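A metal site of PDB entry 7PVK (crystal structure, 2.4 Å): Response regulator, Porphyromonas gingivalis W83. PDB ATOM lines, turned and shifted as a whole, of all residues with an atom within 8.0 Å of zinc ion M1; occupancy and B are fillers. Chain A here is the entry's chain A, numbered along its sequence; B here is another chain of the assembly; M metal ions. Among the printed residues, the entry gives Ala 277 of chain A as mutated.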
ATOM      1  N   ASP A 244      13.163  13.391   2.536  1.00  0.00           N
ATOM      2  CA  ASP A 244      12.550  12.771   3.698  1.00  0.00           C
ATOM      3  C   ASP A 244      13.618  12.341   4.686  1.00  0.00           C
ATOM      4  O   ASP A 244      14.624  11.729   4.308  1.00  0.00           O
ATOM      5  CB  ASP A 244      11.703  11.575   3.263  1.00  0.00           C
ATOM      6  CG  ASP A 244      10.694  11.166   4.320  1.00  0.00           C
ATOM      7  OD1 ASP A 244      11.101  10.994   5.486  1.00  0.00           O
ATOM      8  OD2 ASP A 244       9.493  11.047   3.983  1.00  0.00           O
ATOM      9  N   ASN A 245      13.398  12.670   5.958  1.00  0.00           N
ATOM     10  CA  ASN A 245      14.270  12.240   7.043  1.00  0.00           C
ATOM     11  C   ASN A 245      15.644  12.894   6.925  1.00  0.00           C
ATOM     12  O   ASN A 245      16.664  12.207   6.823  1.00  0.00           O
ATOM     13  CB  ASN A 245      14.401  10.713   7.038  1.00  0.00           C
ATOM     14  CG  ASN A 245      14.733  10.167   8.409  1.00  0.00           C
ATOM     15  OD1 ASN A 245      15.331  10.849   9.238  1.00  0.00           O
ATOM     16  ND2 ASN A 245      14.352   8.916   8.656  1.00  0.00           N
ATOM     17  N   THR A 275       6.119  12.302  14.184  1.00  0.00           N
ATOM     18  CA  THR A 275       7.116  12.758  13.214  1.00  0.00           C
ATOM     19  C   THR A 275       7.334  11.663  12.178  1.00  0.00           C
ATOM     20  O   THR A 275       8.304  10.890  12.210  1.00  0.00           O
ATOM     21  CB  THR A 275       8.418  13.127  13.931  1.00  0.00           C
ATOM     22  OG1 THR A 275       8.742  12.098  14.874  1.00  0.00           O
ATOM     23  CG2 THR A 275       8.255  14.450  14.647  1.00  0.00           C
ATOM     24  N   ALA A 276       6.394  11.579  11.244  1.00  0.00           N
ATOM     25  CA  ALA A 276       6.451  10.629  10.143  1.00  0.00           C
ATOM     26  C   ALA A 276       5.721  11.230   8.949  1.00  0.00           C
ATOM     27  O   ALA A 276       4.950  12.185   9.083  1.00  0.00           O
ATOM     28  CB  ALA A 276       5.837   9.278  10.537  1.00  0.00           C
ATOM     29  N   ALA A 277       5.977  10.668   7.768  1.00  0.00           N
ATOM     30  CA  ALA A 277       5.448  11.247   6.544  1.00  0.00           C
ATOM     31  C   ALA A 277       3.926  11.208   6.489  1.00  0.00           C
ATOM     32  O   ALA A 277       3.309  12.104   5.907  1.00  0.00           O
ATOM     33  CB  ALA A 277       6.029  10.505   5.334  1.00  0.00           C
ATOM     34  N   ASN A 363      13.446  10.205  -1.326  1.00  0.00           N
ATOM     35  CA  ASN A 363      13.176   9.280  -0.231  1.00  0.00           C
ATOM     36  C   ASN A 363      14.355   8.407   0.167  1.00  0.00           C
ATOM     37  O   ASN A 363      14.238   7.666   1.149  1.00  0.00           O
ATOM     38  CB  ASN A 363      11.996   8.357  -0.603  1.00  0.00           C
ATOM     39  CG  ASN A 363      10.659   9.074  -0.553  1.00  0.00           C
ATOM     40  OD1 ASN A 363      10.289   9.629   0.483  1.00  0.00           O
ATOM     41  ND2 ASN A 363       9.931   9.050  -1.667  1.00  0.00           N
ATOM     42  N   VAL A 365      17.126   8.908   1.677  1.00  0.00           N
ATOM     43  CA  VAL A 365      17.671   9.127   3.015  1.00  0.00           C
ATOM     44  C   VAL A 365      16.792   8.467   4.062  1.00  0.00           C
ATOM     45  O   VAL A 365      17.283   7.903   5.048  1.00  0.00           O
ATOM     46  CB  VAL A 365      17.847  10.625   3.282  1.00  0.00           C
ATOM     47  CG1 VAL A 365      18.399  10.868   4.687  1.00  0.00           C
ATOM     48  CG2 VAL A 365      18.784  11.247   2.243  1.00  0.00           C
ATOM     49  N   ASP A 366      15.461   8.521   3.876  1.00  0.00           N
ATOM     50  CA  ASP A 366      14.576   7.801   4.795  1.00  0.00           C
ATOM     51  C   ASP A 366      14.746   6.295   4.625  1.00  0.00           C
ATOM     52  O   ASP A 366      14.779   5.566   5.623  1.00  0.00           O
ATOM     53  CB  ASP A 366      13.131   8.221   4.564  1.00  0.00           C
ATOM     54  CG  ASP A 366      12.147   7.381   5.363  1.00  0.00           C
ATOM     55  OD1 ASP A 366      11.864   7.729   6.529  1.00  0.00           O
ATOM     56  OD2 ASP A 366      11.682   6.351   4.822  1.00  0.00           O
ATOM     57  N   MET A 367      14.858   5.828   3.391  1.00  0.00           N
ATOM     58  CA  MET A 367      15.076   4.417   3.114  1.00  0.00           C
ATOM     59  C   MET A 367      16.356   3.927   3.800  1.00  0.00           C
ATOM     60  O   MET A 367      16.386   2.831   4.358  1.00  0.00           O
ATOM     61  CB  MET A 367      15.160   4.169   1.605  1.00  0.00           C
ATOM     62  CG  MET A 367      13.890   4.540   0.842  1.00  0.00           C
ATOM     63  SD  MET A 367      14.153   4.756  -1.089  1.00  0.00           S
ATOM     64  CE  MET A 367      14.644   2.927  -1.545  1.00  0.00           C
ATOM     65  N   MET A 368      17.393   4.757   3.764  1.00  0.00           N
ATOM     66  CA  MET A 368      18.683   4.417   4.366  1.00  0.00           C
ATOM     67  C   MET A 368      18.611   4.477   5.875  1.00  0.00           C
ATOM     68  O   MET A 368      19.103   3.585   6.572  1.00  0.00           O
ATOM     69  CB  MET A 368      19.776   5.357   3.865  1.00  0.00           C
ATOM     70  CG  MET A 368      21.159   5.008   4.392  1.00  0.00           C
ATOM     71  SD  MET A 368      21.763   6.136   5.865  1.00  0.00           S
ATOM     72  CE  MET A 368      22.325   7.691   4.833  1.00  0.00           C
ATOM     73  N   SER A 369      18.007   5.555   6.401  1.00  0.00           N
ATOM     74  CA  SER A 369      17.821   5.671   7.840  1.00  0.00           C
ATOM     75  C   SER A 369      17.085   4.458   8.391  1.00  0.00           C
ATOM     76  O   SER A 369      17.403   3.984   9.496  1.00  0.00           O
ATOM     77  CB  SER A 369      17.074   6.957   8.166  1.00  0.00           C
ATOM     78  OG  SER A 369      16.799   7.045   9.553  1.00  0.00           O
ATOM     79  N   HIS A 370      16.099   3.946   7.661  1.00  0.00           N
ATOM     80  CA  HIS A 370      15.399   2.752   8.101  1.00  0.00           C
ATOM     81  C   HIS A 370      16.270   1.514   7.950  1.00  0.00           C
ATOM     82  O   HIS A 370      16.233   0.615   8.796  1.00  0.00           O
ATOM     83  CB  HIS A 370      14.109   2.578   7.300  1.00  0.00           C
ATOM     84  CG  HIS A 370      13.013   3.516   7.715  1.00  0.00           C
ATOM     85  ND1 HIS A 370      12.419   3.466   8.959  1.00  0.00           N
ATOM     86  CD2 HIS A 370      12.414   4.530   7.046  1.00  0.00           C
ATOM     87  CE1 HIS A 370      11.501   4.409   9.034  1.00  0.00           C
ATOM     88  NE2 HIS A 370      11.472   5.064   7.889  1.00  0.00           N
ATOM     89  N   ASP A 420      10.469  16.605   6.117  1.00  0.00           N
ATOM     90  CA  ASP A 420       9.241  16.388   6.873  1.00  0.00           C
ATOM     91  C   ASP A 420       9.476  15.986   8.318  1.00  0.00           C
ATOM     92  O   ASP A 420       8.559  16.111   9.135  1.00  0.00           O
ATOM     93  CB  ASP A 420       8.389  15.294   6.198  1.00  0.00           C
ATOM     94  CG  ASP A 420       9.126  13.986   6.060  1.00  0.00           C
ATOM     95  OD1 ASP A 420      10.380  13.988   6.035  1.00  0.00           O
ATOM     96  OD2 ASP A 420       8.457  12.932   5.993  1.00  0.00           O
ATOM     97  N   HIS A 421      10.673  15.510   8.650  1.00  0.00           N
ATOM     98  CA  HIS A 421      10.991  15.081  10.009  1.00  0.00           C
ATOM     99  C   HIS A 421      12.457  14.668  10.012  1.00  0.00           C
ATOM    100  O   HIS A 421      13.083  14.493   8.962  1.00  0.00           O
ATOM    101  CB  HIS A 421      10.111  13.926  10.466  1.00  0.00           C
ATOM    102  CG  HIS A 421      10.235  12.700   9.617  1.00  0.00           C
ATOM    103  ND1 HIS A 421      11.276  11.805   9.740  1.00  0.00           N
ATOM    104  CD2 HIS A 421       9.443  12.224   8.617  1.00  0.00           C
ATOM    105  CE1 HIS A 421      11.120  10.832   8.858  1.00  0.00           C
ATOM    106  NE2 HIS A 421      10.021  11.055   8.169  1.00  0.00           N
ATOM    107  N   GLY A 422      13.004  14.531  11.214  1.00  0.00           N
ATOM    108  CA  GLY A 422      14.327  14.008  11.410  1.00  0.00           C
ATOM    109  C   GLY A 422      14.308  12.558  11.853  1.00  0.00           C
ATOM    110  O   GLY A 422      13.394  11.795  11.507  1.00  0.00           O
ATOM    111  N   THR A 423      15.329  12.173  12.604  1.00  0.00           N
ATOM    112  CA  THR A 423      15.377  10.850  13.222  1.00  0.00           C
ATOM    113  C   THR A 423      16.417  10.897  14.323  1.00  0.00           C
ATOM    114  O   THR A 423      17.312  11.743  14.330  1.00  0.00           O
ATOM    115  CB  THR A 423      15.714   9.755  12.205  1.00  0.00           C
ATOM    116  OG1 THR A 423      15.269   8.485  12.704  1.00  0.00           O
ATOM    117  CG2 THR A 423      17.218   9.680  11.916  1.00  0.00           C
ATOM    118  N   ASN A 441       5.366   1.156  14.484  1.00  0.00           N
ATOM    119  CA  ASN A 441       6.338   2.214  14.718  1.00  0.00           C
ATOM    120  C   ASN A 441       6.816   2.160  16.166  1.00  0.00           C
ATOM    121  O   ASN A 441       6.057   1.824  17.087  1.00  0.00           O
ATOM    122  CB  ASN A 441       5.715   3.585  14.417  1.00  0.00           C
ATOM    123  CG  ASN A 441       6.705   4.720  14.556  1.00  0.00           C
ATOM    124  OD1 ASN A 441       7.352   4.881  15.596  1.00  0.00           O
ATOM    125  ND2 ASN A 441       6.837   5.505  13.506  1.00  0.00           N
ATOM    126  N   PHE A 503      18.093   4.161  14.183  1.00  0.00           N
ATOM    127  CA  PHE A 503      17.455   5.453  13.931  1.00  0.00           C
ATOM    128  C   PHE A 503      15.950   5.242  13.797  1.00  0.00           C
ATOM    129  O   PHE A 503      15.497   4.425  12.991  1.00  0.00           O
ATOM    130  CB  PHE A 503      18.032   6.103  12.682  1.00  0.00           C
ATOM    131  CG  PHE A 503      19.512   6.372  12.765  1.00  0.00           C
ATOM    132  CD1 PHE A 503      20.023   7.151  13.789  1.00  0.00           C
ATOM    133  CD2 PHE A 503      20.379   5.853  11.824  1.00  0.00           C
ATOM    134  CE1 PHE A 503      21.382   7.402  13.867  1.00  0.00           C
ATOM    135  CE2 PHE A 503      21.738   6.104  11.901  1.00  0.00           C
ATOM    136  CZ  PHE A 503      22.239   6.874  12.921  1.00  0.00           C
ATOM    137  N   GLN A 504      15.178   5.979  14.603  1.00  0.00           N
ATOM    138  CA  GLN A 504      13.732   5.871  14.599  1.00  0.00           C
ATOM    139  C   GLN A 504      13.141   7.267  14.688  1.00  0.00           C
ATOM    140  O   GLN A 504      13.606   8.092  15.476  1.00  0.00           O
ATOM    141  CB  GLN A 504      13.221   5.019  15.757  1.00  0.00           C
ATOM    142  CG  GLN A 504      13.815   3.622  15.812  1.00  0.00           C
ATOM    143  CD  GLN A 504      13.482   2.805  14.582  1.00  0.00           C
ATOM    144  OE1 GLN A 504      12.602   3.166  13.807  1.00  0.00           O
ATOM    145  NE2 GLN A 504      14.199   1.698  14.394  1.00  0.00           N
ATOM    146  N   HIS A 505      12.107   7.516  13.894  1.00  0.00           N
ATOM    147  CA  HIS A 505      11.363   8.760  13.935  1.00  0.00           C
ATOM    148  C   HIS A 505       9.903   8.467  14.252  1.00  0.00           C
ATOM    149  O   HIS A 505       9.458   7.316  14.220  1.00  0.00           O
ATOM    150  CB  HIS A 505      11.498   9.539  12.616  1.00  0.00           C
ATOM    151  CG  HIS A 505      11.035   8.773  11.424  1.00  0.00           C
ATOM    152  ND1 HIS A 505       9.774   8.916  10.886  1.00  0.00           N
ATOM    153  CD2 HIS A 505      11.668   7.859  10.646  1.00  0.00           C
ATOM    154  CE1 HIS A 505       9.654   8.134   9.831  1.00  0.00           C
ATOM    155  NE2 HIS A 505      10.789   7.472   9.672  1.00  0.00           N
ATOM    156  N   GLY A 506       9.168   9.528  14.561  1.00  0.00           N
ATOM    157  CA  GLY A 506       7.781   9.431  14.975  1.00  0.00           C
ATOM    158  C   GLY A 506       7.514   9.970  16.366  1.00  0.00           C
ATOM    159  O   GLY A 506       6.358  10.274  16.698  1.00  0.00           O
ATOM    160  P     G B   1       8.273   7.859   6.703  1.00  0.00           P
ATOM    161  OP1   G B   1       7.273   8.166   7.746  1.00  0.00           O
ATOM    162  OP2   G B   1       9.057   6.691   7.156  1.00  0.00           O
ATOM    163  O5'   G B   1       7.518   7.398   5.392  1.00  0.00           O
ATOM    164  C5'   G B   1       8.251   7.032   4.226  1.00  0.00           C
ATOM    165  C4'   G B   1       7.343   6.505   3.128  1.00  0.00           C
ATOM    166  O4'   G B   1       6.830   5.209   3.544  1.00  0.00           O
ATOM    167  C3'   G B   1       6.130   7.390   2.822  1.00  0.00           C
ATOM    168  O3'   G B   1       5.810   7.451   1.422  1.00  0.00           O
ATOM    169  C2'   G B   1       4.993   6.676   3.571  1.00  0.00           C
ATOM    170  O2'   G B   1       3.716   6.868   3.000  1.00  0.00           O
ATOM    171  C1'   G B   1       5.422   5.215   3.463  1.00  0.00           C
ATOM    172  N9    G B   1       4.885   4.362   4.530  1.00  0.00           N
ATOM    173  C8    G B   1       5.027   4.549   5.881  1.00  0.00           C
ATOM    174  N7    G B   1       4.435   3.624   6.589  1.00  0.00           N
ATOM    175  C5    G B   1       3.877   2.777   5.640  1.00  0.00           C
ATOM    176  C6    G B   1       3.111   1.585   5.800  1.00  0.00           C
ATOM    177  O6    G B   1       2.768   1.019   6.839  1.00  0.00           O
ATOM    178  N1    G B   1       2.750   1.047   4.567  1.00  0.00           N
ATOM    179  C2    G B   1       3.070   1.574   3.353  1.00  0.00           C
ATOM    180  N2    G B   1       2.635   0.907   2.276  1.00  0.00           N
ATOM    181  N3    G B   1       3.783   2.683   3.184  1.00  0.00           N
ATOM    182  C4    G B   1       4.148   3.225   4.363  1.00  0.00           C
ATOM    183  P     G B   2       6.889   7.210   0.261  1.00  0.00           P
ATOM    184  OP1   G B   2       8.231   7.701   0.673  1.00  0.00           O
ATOM    185  OP2   G B   2       6.300   7.768  -0.989  1.00  0.00           O
ATOM    186  O5'   G B   2       6.884   5.627   0.120  1.00  0.00           O
ATOM    187  C5'   G B   2       8.011   4.910  -0.366  1.00  0.00           C
ATOM    188  C4'   G B   2       7.592   3.624  -1.025  1.00  0.00           C
ATOM    189  O4'   G B   2       6.355   3.861  -1.761  1.00  0.00           O
ATOM    190  C3'   G B   2       8.581   3.045  -2.031  1.00  0.00           C
ATOM    191  O3'   G B   2       8.534   1.619  -2.011  1.00  0.00           O
ATOM    192  C2'   G B   2       8.055   3.559  -3.375  1.00  0.00           C
ATOM    193  O2'   G B   2       8.397   2.735  -4.474  1.00  0.00           O
ATOM    194  C1'   G B   2       6.541   3.571  -3.139  1.00  0.00           C
ATOM    195  N9    G B   2       5.827   4.591  -3.912  1.00  0.00           N
ATOM    196  C8    G B   2       5.525   5.857  -3.465  1.00  0.00           C
ATOM    197  N7    G B   2       4.874   6.573  -4.345  1.00  0.00           N
ATOM    198  C5    G B   2       4.713   5.725  -5.423  1.00  0.00           C
ATOM    199  C6    G B   2       4.082   5.954  -6.676  1.00  0.00           C
ATOM    200  O6    G B   2       3.510   6.972  -7.075  1.00  0.00           O
ATOM    201  N1    G B   2       4.148   4.834  -7.490  1.00  0.00           N
ATOM    202  C2    G B   2       4.746   3.648  -7.158  1.00  0.00           C
ATOM    203  N2    G B   2       4.694   2.687  -8.094  1.00  0.00           N
ATOM    204  N3    G B   2       5.342   3.419  -5.996  1.00  0.00           N
ATOM    205  C4    G B   2       5.284   4.494  -5.180  1.00  0.00           C
HETATM  206 ZN    ZN M   1      10.942   6.976   7.773  1.00  0.00          ZN
HETATM  207 ZN    ZN M   2       9.436  11.002   6.342  1.00  0.00          ZN
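N of Ala 277 lies within hydrogen-bond range of OP1 of G 1 of chain B (2.8 Å). The side-chain amide nitrogen (ND2) of Asn 441 sits at hydrogen-bond distance from the backbone carbonyl oxygen (O) of His 505. The side-chain amide nitrogen (ND2) of Asn 245 sits close to the side-chain carboxylate (OD1) of Asp 366 (3.5 Å). ND1 of His 505 is in hydrogen-bond range of O of Thr 275 (2.8 Å). O of Asp 244 sits at hydrogen-bond distance from N of Asp 366, 3.3 Å away. A ring nitrogen (ND1) of His 505 sits close to a ring nitrogen (ND1) of His 421 (3.5 Å).
Four residues have an atom within 4 Å of zinc ion M1: Asp 366, His 370, His 505 and G 1 of chain B. The nearest printed residue that does not touch zinc ion M1 is His 421 (4.01 Å).
Zinc ion M1 is bound by OD1 of Asp 366 (1.7 Å), NE2 of His 505 (2.0 Å), NE2 of His 370 (2.0 Å) and OP2 of G 1 of chain B (2.0 Å).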
